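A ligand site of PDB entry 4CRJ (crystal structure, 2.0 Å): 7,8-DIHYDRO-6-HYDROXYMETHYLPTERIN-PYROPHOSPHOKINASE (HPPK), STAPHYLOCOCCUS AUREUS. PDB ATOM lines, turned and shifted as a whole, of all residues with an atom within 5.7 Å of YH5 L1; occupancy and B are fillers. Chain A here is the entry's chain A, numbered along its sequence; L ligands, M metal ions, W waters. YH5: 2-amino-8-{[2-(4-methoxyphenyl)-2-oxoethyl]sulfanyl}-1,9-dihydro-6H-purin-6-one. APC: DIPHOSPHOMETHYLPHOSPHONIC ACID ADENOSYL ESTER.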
ATOM      1  N   LEU A  11      14.917 -14.390  34.255  1.00  0.00           N
ATOM      2  CA  LEU A  11      15.108 -15.610  35.022  1.00  0.00           C
ATOM      3  C   LEU A  11      13.923 -16.547  34.825  1.00  0.00           C
ATOM      4  O   LEU A  11      12.785 -16.119  34.784  1.00  0.00           O
ATOM      5  CB  LEU A  11      15.235 -15.289  36.516  1.00  0.00           C
ATOM      6  CG  LEU A  11      16.616 -14.830  36.979  1.00  0.00           C
ATOM      7  CD1 LEU A  11      16.974 -13.472  36.428  1.00  0.00           C
ATOM      8  CD2 LEU A  11      16.660 -14.799  38.499  1.00  0.00           C
ATOM      9  N   GLY A  12      14.223 -17.847  34.723  1.00  0.00           N
ATOM     10  CA  GLY A  12      13.203 -18.865  34.551  1.00  0.00           C
ATOM     11  C   GLY A  12      13.547 -20.118  35.314  1.00  0.00           C
ATOM     12  O   GLY A  12      14.723 -20.420  35.518  1.00  0.00           O
ATOM     13  N   SER A  13      12.519 -20.847  35.727  1.00  0.00           N
ATOM     14  CA  SER A  13      12.712 -22.152  36.380  1.00  0.00           C
ATOM     15  C   SER A  13      11.479 -22.988  36.138  1.00  0.00           C
ATOM     16  O   SER A  13      10.365 -22.503  36.336  1.00  0.00           O
ATOM     17  CB  SER A  13      12.948 -21.983  37.884  1.00  0.00           C
ATOM     18  OG  SER A  13      13.089 -23.267  38.524  1.00  0.00           O
ATOM     19  N   THR A  46       4.003 -19.381  33.850  1.00  0.00           N
ATOM     20  CA  THR A  46       3.896 -19.321  32.406  1.00  0.00           C
ATOM     21  C   THR A  46       3.915 -20.703  31.782  1.00  0.00           C
ATOM     22  O   THR A  46       4.678 -21.590  32.192  1.00  0.00           O
ATOM     23  CB  THR A  46       5.009 -18.411  31.817  1.00  0.00           C
ATOM     24  OG1 THR A  46       6.301 -18.953  32.102  1.00  0.00           O
ATOM     25  CG2 THR A  46       4.949 -17.014  32.416  1.00  0.00           C
ATOM     26  N   ALA A  47       3.015 -20.904  30.824  1.00  0.00           N
ATOM     27  CA  ALA A  47       2.992 -22.138  30.052  1.00  0.00           C
ATOM     28  C   ALA A  47       4.307 -22.235  29.281  1.00  0.00           C
ATOM     29  O   ALA A  47       4.806 -21.218  28.805  1.00  0.00           O
ATOM     30  CB  ALA A  47       1.831 -22.145  29.091  1.00  0.00           C
ATOM     31  N   PRO A  48       4.872 -23.445  29.158  1.00  0.00           N
ATOM     32  CA  PRO A  48       6.151 -23.566  28.475  1.00  0.00           C
ATOM     33  C   PRO A  48       5.970 -23.267  27.010  1.00  0.00           C
ATOM     34  O   PRO A  48       4.962 -23.657  26.424  1.00  0.00           O
ATOM     35  CB  PRO A  48       6.550 -25.031  28.689  1.00  0.00           C
ATOM     36  CG  PRO A  48       5.288 -25.749  29.012  1.00  0.00           C
ATOM     37  CD  PRO A  48       4.242 -24.747  29.425  1.00  0.00           C
ATOM     38  N   VAL A  49       6.924 -22.536  26.446  1.00  0.00           N
ATOM     39  CA  VAL A  49       6.920 -22.149  25.036  1.00  0.00           C
ATOM     40  C   VAL A  49       8.015 -22.948  24.310  1.00  0.00           C
ATOM     41  O   VAL A  49       9.106 -23.173  24.857  1.00  0.00           O
ATOM     42  CB  VAL A  49       7.170 -20.632  24.868  1.00  0.00           C
ATOM     43  CG1 VAL A  49       7.002 -20.211  23.412  1.00  0.00           C
ATOM     44  CG2 VAL A  49       6.219 -19.831  25.743  1.00  0.00           C
ATOM     45  N   GLY A  50       7.712 -23.375  23.087  1.00  0.00           N
ATOM     46  CA  GLY A  50       8.618 -24.224  22.316  1.00  0.00           C
ATOM     47  C   GLY A  50       8.246 -25.672  22.557  1.00  0.00           C
ATOM     48  O   GLY A  50       7.235 -26.149  22.032  1.00  0.00           O
ATOM     49  N   TYR A  51       9.060 -26.378  23.328  1.00  0.00           N
ATOM     50  CA  TYR A  51       8.728 -27.740  23.733  1.00  0.00           C
ATOM     51  C   TYR A  51       7.644 -27.665  24.808  1.00  0.00           C
ATOM     52  O   TYR A  51       7.857 -27.126  25.887  1.00  0.00           O
ATOM     53  CB  TYR A  51       9.977 -28.457  24.256  1.00  0.00           C
ATOM     54  CG  TYR A  51       9.750 -29.906  24.655  1.00  0.00           C
ATOM     55  CD1 TYR A  51       9.032 -30.779  23.826  1.00  0.00           C
ATOM     56  CD2 TYR A  51      10.255 -30.411  25.850  1.00  0.00           C
ATOM     57  CE1 TYR A  51       8.828 -32.105  24.192  1.00  0.00           C
ATOM     58  CE2 TYR A  51      10.070 -31.736  26.216  1.00  0.00           C
ATOM     59  CZ  TYR A  51       9.351 -32.578  25.383  1.00  0.00           C
ATOM     60  OH  TYR A  51       9.155 -33.894  25.752  1.00  0.00           O
ATOM     61  N   GLN A  54       6.768 -30.212  28.883  1.00  0.00           N
ATOM     62  CA  GLN A  54       7.670 -29.988  30.000  1.00  0.00           C
ATOM     63  C   GLN A  54       6.919 -29.112  30.987  1.00  0.00           C
ATOM     64  O   GLN A  54       5.841 -28.635  30.677  1.00  0.00           O
ATOM     65  CB  GLN A  54       8.972 -29.326  29.537  1.00  0.00           C
ATOM     66  CG  GLN A  54       8.806 -27.922  28.990  1.00  0.00           C
ATOM     67  CD  GLN A  54      10.142 -27.248  28.693  1.00  0.00           C
ATOM     68  OE1 GLN A  54      11.093 -27.334  29.486  1.00  0.00           O
ATOM     69  NE2 GLN A  54      10.210 -26.565  27.559  1.00  0.00           N
ATOM     70  N   PHE A  57       6.603 -22.885  33.781  1.00  0.00           N
ATOM     71  CA  PHE A  57       7.685 -22.083  34.299  1.00  0.00           C
ATOM     72  C   PHE A  57       7.199 -21.081  35.326  1.00  0.00           C
ATOM     73  O   PHE A  57       6.042 -20.658  35.304  1.00  0.00           O
ATOM     74  CB  PHE A  57       8.338 -21.287  33.156  1.00  0.00           C
ATOM     75  CG  PHE A  57       9.278 -22.081  32.294  1.00  0.00           C
ATOM     76  CD1 PHE A  57       8.785 -22.922  31.297  1.00  0.00           C
ATOM     77  CD2 PHE A  57      10.659 -21.958  32.448  1.00  0.00           C
ATOM     78  CE1 PHE A  57       9.652 -23.630  30.490  1.00  0.00           C
ATOM     79  CE2 PHE A  57      11.526 -22.664  31.631  1.00  0.00           C
ATOM     80  CZ  PHE A  57      11.022 -23.499  30.647  1.00  0.00           C
ATOM     81  N   ASN A  59       8.665 -17.306  35.819  1.00  0.00           N
ATOM     82  CA  ASN A  59       9.521 -16.328  35.154  1.00  0.00           C
ATOM     83  C   ASN A  59       9.456 -14.970  35.867  1.00  0.00           C
ATOM     84  O   ASN A  59       8.397 -14.568  36.372  1.00  0.00           O
ATOM     85  CB  ASN A  59       9.106 -16.132  33.685  1.00  0.00           C
ATOM     86  CG  ASN A  59       9.562 -17.248  32.776  1.00  0.00           C
ATOM     87  OD1 ASN A  59       8.755 -17.996  32.217  1.00  0.00           O
ATOM     88  ND2 ASN A  59      10.876 -17.369  32.606  1.00  0.00           N
ATOM     89  N   ARG A  91      18.801 -27.071  25.072  1.00  0.00           N
ATOM     90  CA  ARG A  91      18.223 -25.731  25.001  1.00  0.00           C
ATOM     91  C   ARG A  91      16.694 -25.769  25.058  1.00  0.00           C
ATOM     92  O   ARG A  91      16.061 -24.903  25.647  1.00  0.00           O
ATOM     93  CB  ARG A  91      18.665 -25.015  23.723  1.00  0.00           C
ATOM     94  CG  ARG A  91      20.160 -24.727  23.646  1.00  0.00           C
ATOM     95  CD  ARG A  91      20.516 -24.121  22.294  1.00  0.00           C
ATOM     96  NE  ARG A  91      19.857 -22.830  22.111  1.00  0.00           N
ATOM     97  CZ  ARG A  91      20.418 -21.643  22.344  1.00  0.00           C
ATOM     98  NH1 ARG A  91      21.688 -21.558  22.752  1.00  0.00           N
ATOM     99  NH2 ARG A  91      19.709 -20.538  22.149  1.00  0.00           N
ATOM    100  N   TRP A  92      16.120 -26.783  24.415  1.00  0.00           N
ATOM    101  CA  TRP A  92      14.664 -26.941  24.347  1.00  0.00           C
ATOM    102  C   TRP A  92      14.055 -27.540  25.619  1.00  0.00           C
ATOM    103  O   TRP A  92      12.835 -27.489  25.798  1.00  0.00           O
ATOM    104  CB  TRP A  92      14.275 -27.807  23.134  1.00  0.00           C
ATOM    105  CG  TRP A  92      14.990 -29.137  23.068  1.00  0.00           C
ATOM    106  CD1 TRP A  92      16.116 -29.427  22.331  1.00  0.00           C
ATOM    107  CD2 TRP A  92      14.637 -30.344  23.759  1.00  0.00           C
ATOM    108  NE1 TRP A  92      16.486 -30.726  22.534  1.00  0.00           N
ATOM    109  CE2 TRP A  92      15.593 -31.321  23.397  1.00  0.00           C
ATOM    110  CE3 TRP A  92      13.612 -30.694  24.645  1.00  0.00           C
ATOM    111  CZ2 TRP A  92      15.552 -32.631  23.894  1.00  0.00           C
ATOM    112  CZ3 TRP A  92      13.569 -31.993  25.145  1.00  0.00           C
ATOM    113  CH2 TRP A  92      14.533 -32.944  24.759  1.00  0.00           C
ATOM    114  N   GLY A  93      14.894 -28.103  26.486  1.00  0.00           N
ATOM    115  CA  GLY A  93      14.442 -28.915  27.606  1.00  0.00           C
ATOM    116  C   GLY A  93      14.317 -28.146  28.900  1.00  0.00           C
ATOM    117  O   GLY A  93      14.675 -26.981  28.972  1.00  0.00           O
ATOM    118  N   ARG A  95      14.771 -26.915  32.970  1.00  0.00           N
ATOM    119  CA  ARG A  95      15.933 -26.491  33.743  1.00  0.00           C
ATOM    120  C   ARG A  95      15.553 -25.942  35.129  1.00  0.00           C
ATOM    121  O   ARG A  95      14.508 -25.272  35.297  1.00  0.00           O
ATOM    122  CB  ARG A  95      16.784 -25.466  32.966  1.00  0.00           C
ATOM    123  CG  ARG A  95      16.189 -24.064  32.808  1.00  0.00           C
ATOM    124  CD  ARG A  95      14.977 -24.030  31.880  1.00  0.00           C
ATOM    125  NE  ARG A  95      15.291 -24.614  30.581  1.00  0.00           N
ATOM    126  CZ  ARG A  95      15.803 -23.941  29.538  1.00  0.00           C
ATOM    127  NH1 ARG A  95      16.053 -22.637  29.607  1.00  0.00           N
ATOM    128  NH2 ARG A  95      16.077 -24.599  28.408  1.00  0.00           N
ATOM    129  N   ASP A  98      17.408 -20.697  34.664  1.00  0.00           N
ATOM    130  CA  ASP A  98      17.867 -20.087  33.402  1.00  0.00           C
ATOM    131  C   ASP A  98      18.022 -18.600  33.674  1.00  0.00           C
ATOM    132  O   ASP A  98      17.110 -17.966  34.187  1.00  0.00           O
ATOM    133  CB  ASP A  98      16.825 -20.324  32.308  1.00  0.00           C
ATOM    134  CG  ASP A  98      17.256 -19.786  30.957  1.00  0.00           C
ATOM    135  OD1 ASP A  98      18.462 -19.855  30.641  1.00  0.00           O
ATOM    136  OD2 ASP A  98      16.394 -19.301  30.196  1.00  0.00           O
ATOM    137  N   ARG A 124       8.090 -12.899  23.277  1.00  0.00           N
ATOM    138  CA  ARG A 124       7.871 -13.720  24.478  1.00  0.00           C
ATOM    139  C   ARG A 124       7.148 -12.937  25.554  1.00  0.00           C
ATOM    140  O   ARG A 124       7.730 -12.075  26.192  1.00  0.00           O
ATOM    141  CB  ARG A 124       9.189 -14.238  25.005  1.00  0.00           C
ATOM    142  CG  ARG A 124       9.850 -15.252  24.101  1.00  0.00           C
ATOM    143  CD  ARG A 124      11.244 -15.550  24.586  1.00  0.00           C
ATOM    144  NE  ARG A 124      11.858 -16.678  23.884  1.00  0.00           N
ATOM    145  CZ  ARG A 124      13.030 -17.205  24.209  1.00  0.00           C
ATOM    146  NH1 ARG A 124      13.735 -16.730  25.231  1.00  0.00           N
ATOM    147  NH2 ARG A 124      13.506 -18.212  23.490  1.00  0.00           N
ATOM    148  N   PHE A 126       6.324 -14.068  28.365  1.00  0.00           N
ATOM    149  CA  PHE A 126       6.944 -14.425  29.651  1.00  0.00           C
ATOM    150  C   PHE A 126       8.190 -13.595  29.963  1.00  0.00           C
ATOM    151  O   PHE A 126       8.696 -13.620  31.089  1.00  0.00           O
ATOM    152  CB  PHE A 126       7.213 -15.942  29.755  1.00  0.00           C
ATOM    153  CG  PHE A 126       8.338 -16.456  28.881  1.00  0.00           C
ATOM    154  CD1 PHE A 126       9.660 -16.253  29.243  1.00  0.00           C
ATOM    155  CD2 PHE A 126       8.064 -17.189  27.736  1.00  0.00           C
ATOM    156  CE1 PHE A 126      10.696 -16.731  28.453  1.00  0.00           C
ATOM    157  CE2 PHE A 126       9.091 -17.691  26.962  1.00  0.00           C
ATOM    158  CZ  PHE A 126      10.413 -17.469  27.329  1.00  0.00           C
HETATM  159  C1  YH5 L   1      10.765 -19.818  29.668  1.00  0.00           C
HETATM  160  O1  YH5 L   1      11.743 -19.182  30.377  1.00  0.00           O
HETATM  161  N1  YH5 L   1      12.249 -21.042  28.059  1.00  0.00           N
HETATM  162  S1  YH5 L   1      12.971 -22.678  26.003  1.00  0.00           S
HETATM  163  C10 YH5 L   1      11.494 -22.418  21.032  1.00  0.00           C
HETATM  164  C11 YH5 L   1      10.362 -21.775  20.578  1.00  0.00           C
HETATM  165  C12 YH5 L   1       9.761 -20.821  21.362  1.00  0.00           C
HETATM  166  C13 YH5 L   1      10.281 -20.499  22.591  1.00  0.00           C
HETATM  167  C14 YH5 L   1      10.315 -23.052  18.632  1.00  0.00           C
HETATM  168  N2  YH5 L   1      10.538 -22.009  26.993  1.00  0.00           N
HETATM  169  C2  YH5 L   1      11.062 -20.659  28.616  1.00  0.00           C
HETATM  170  O2  YH5 L   1      11.192 -19.929  24.987  1.00  0.00           O
HETATM  171  N3  YH5 L   1       8.720 -21.080  28.266  1.00  0.00           N
HETATM  172  C3  YH5 L   1      11.895 -21.854  27.095  1.00  0.00           C
HETATM  173  O3  YH5 L   1       9.717 -22.004  19.366  1.00  0.00           O
HETATM  174  C4  YH5 L   1      10.003 -21.244  27.974  1.00  0.00           C
HETATM  175  N4  YH5 L   1       9.491 -19.609  29.990  1.00  0.00           N
HETATM  176  C5  YH5 L   1       8.544 -20.247  29.290  1.00  0.00           C
HETATM  177  N5  YH5 L   1       7.248 -20.000  29.664  1.00  0.00           N
HETATM  178  C6  YH5 L   1      13.208 -21.229  24.933  1.00  0.00           C
HETATM  179  C7  YH5 L   1      11.900 -20.722  24.372  1.00  0.00           C
HETATM  180  C8  YH5 L   1      11.412 -21.130  23.038  1.00  0.00           C
HETATM  181  C9  YH5 L   1      12.034 -22.097  22.271  1.00  0.00           C
HETATM  182  PG  APC L   2      16.892 -18.579  25.117  1.00  0.00           P
HETATM  183  O1G APC L   2      15.860 -18.202  26.150  1.00  0.00           O
HETATM  184  O2G APC L   2      16.377 -18.389  23.693  1.00  0.00           O
HETATM  185  O3G APC L   2      18.237 -17.965  25.362  1.00  0.00           O
HETATM  186  PB  APC L   2      17.832 -20.788  26.579  1.00  0.00           P
HETATM  187  O1B APC L   2      17.849 -19.790  27.686  1.00  0.00           O
HETATM  188  O2B APC L   2      16.973 -22.081  26.931  1.00  0.00           O
HETATM  189  O3B APC L   2      17.105 -20.152  25.272  1.00  0.00           O
HETATM  190  PA  APC L   2      20.549 -21.855  27.313  1.00  0.00           P
HETATM  191  O1A APC L   2      20.311 -21.066  28.546  1.00  0.00           O
HETATM  192  O2A APC L   2      20.423 -23.423  27.504  1.00  0.00           O
HETATM  193  C3A APC L   2      19.465 -21.286  25.995  1.00  0.00           C
HETATM  194  O5' APC L   2      22.034 -21.650  26.773  1.00  0.00           O
HETATM  195  C5' APC L   2      22.830 -20.597  27.221  1.00  0.00           C
HETATM  196  C4' APC L   2      23.694 -20.195  26.045  1.00  0.00           C
HETATM  197  O4' APC L   2      23.007 -19.341  25.118  1.00  0.00           O
HETATM  198  C3' APC L   2      24.840 -19.423  26.615  1.00  0.00           C
HETATM  199  O3' APC L   2      25.873 -20.359  26.898  1.00  0.00           O
HETATM  200  C2' APC L   2      25.140 -18.374  25.548  1.00  0.00           C
HETATM  201  O2' APC L   2      26.301 -18.759  24.786  1.00  0.00           O
HETATM  202  C1' APC L   2      23.899 -18.341  24.663  1.00  0.00           C
HETATM  203  N9  APC L   2      23.283 -16.988  24.699  1.00  0.00           N
HETATM  204  C8  APC L   2      23.106 -16.221  23.595  1.00  0.00           C
HETATM  205  N7  APC L   2      22.548 -15.037  23.907  1.00  0.00           N
HETATM  206  C5  APC L   2      22.358 -15.034  25.245  1.00  0.00           C
HETATM  207  C6  APC L   2      21.792 -14.075  26.224  1.00  0.00           C
HETATM  208  N6  APC L   2      21.341 -12.885  25.781  1.00  0.00           N
HETATM  209  N1  APC L   2      21.753 -14.452  27.545  1.00  0.00           N
HETATM  210  C2  APC L   2      22.213 -15.653  27.954  1.00  0.00           C
HETATM  211  N3  APC L   2      22.740 -16.563  27.102  1.00  0.00           N
HETATM  212  C4  APC L   2      22.827 -16.324  25.766  1.00  0.00           C
HETATM  213 MG    MG M   1      16.037 -18.675  28.160  1.00  0.00          MG
HETATM  214  O   HOH W   1      14.135 -17.871  28.747  1.00  0.00           O
HETATM  215  O   HOH W   2      13.971 -20.703  30.971  1.00  0.00           O
HETATM  216  O   HOH W   3      14.943 -20.452  27.786  1.00  0.00           O
HETATM  217  O   HOH W   4      11.400 -25.351  24.402  1.00  0.00           O
HETATM  218  O   HOH W   5      15.856 -22.646  24.051  1.00  0.00           O
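Merely in contact with YH5 L1: Phe 126, Phe 57, Gly 50, Pro 48 and Arg 91.
Hydrophobic or aromatic side chains within 4 Å of YH5 L1: Val 49, Phe 57 and Phe 126.
Within 4 Å of YH5 L1: Thr 46, Ala 47, Pro 48, Val 49, Gly 50, Phe 57, Asn 59, Arg 91, Arg 124 and Phe 126.
A nitrogen (N5) of YH5 L1 lies within hydrogen-bond range of the backbone carbonyl oxygen (O) of Ala 47 (2.9 Å).
NH1 of Arg 95 lies within salt-bridge range of O2B of APC L2, at 2.9 Å.
NH2 of Arg 124 is in salt-bridge range of O2G of APC L2 (2.9 Å).
The backbone NH of Val 49 lies within hydrogen-bond range of a nitrogen (N3) of YH5 L1 (2.9 Å).
An oxygen (O4') of APC L2 sits at hydrogen-bond distance from the guanidinium group of Arg 91 (3.5 Å).
The guanidinium group (NH2) of Arg 124 sits close to an oxygen (O2) of YH5 L1, at 3.2 Å.
The backbone carbonyl oxygen (O) of Val 49 is in hydrogen-bond range of a nitrogen (N2) of YH5 L1, 2.8 Å away.
N4 of YH5 L1 sits at hydrogen-bond distance from OD1 of Asn 59, 2.8 Å away.
OG1 of Thr 46 sits at hydrogen-bond distance from N5 of YH5 L1 (2.8 Å).
Water W2 lies within hydrogen-bond range of an oxygen (O1) of YH5 L1 (2.8 Å) and the guanidinium group (NH1) of Arg 95 (3.2 Å).
Water W3 lies within hydrogen-bond range of O2B of APC L2 (2.7 Å), N1 of YH5 L1 (2.8 Å) and NH1 of Arg 95 (3.1 Å).
O of Thr 46 sits at hydrogen-bond distance from N of Phe 57, 2.8 Å away.
The backbone carbonyl oxygen of Arg 91 lies within hydrogen-bond range of the guanidinium group of Arg 95.
The side-chain amide nitrogen of Asn 59 lies within hydrogen-bond range of the backbone carbonyl oxygen of Leu 11 (3.2 Å).
The side-chain hydroxyl (OG1) of Thr 46 lies within hydrogen-bond range of the side-chain amide oxygen (OD1) of Asn 59 (2.6 Å).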
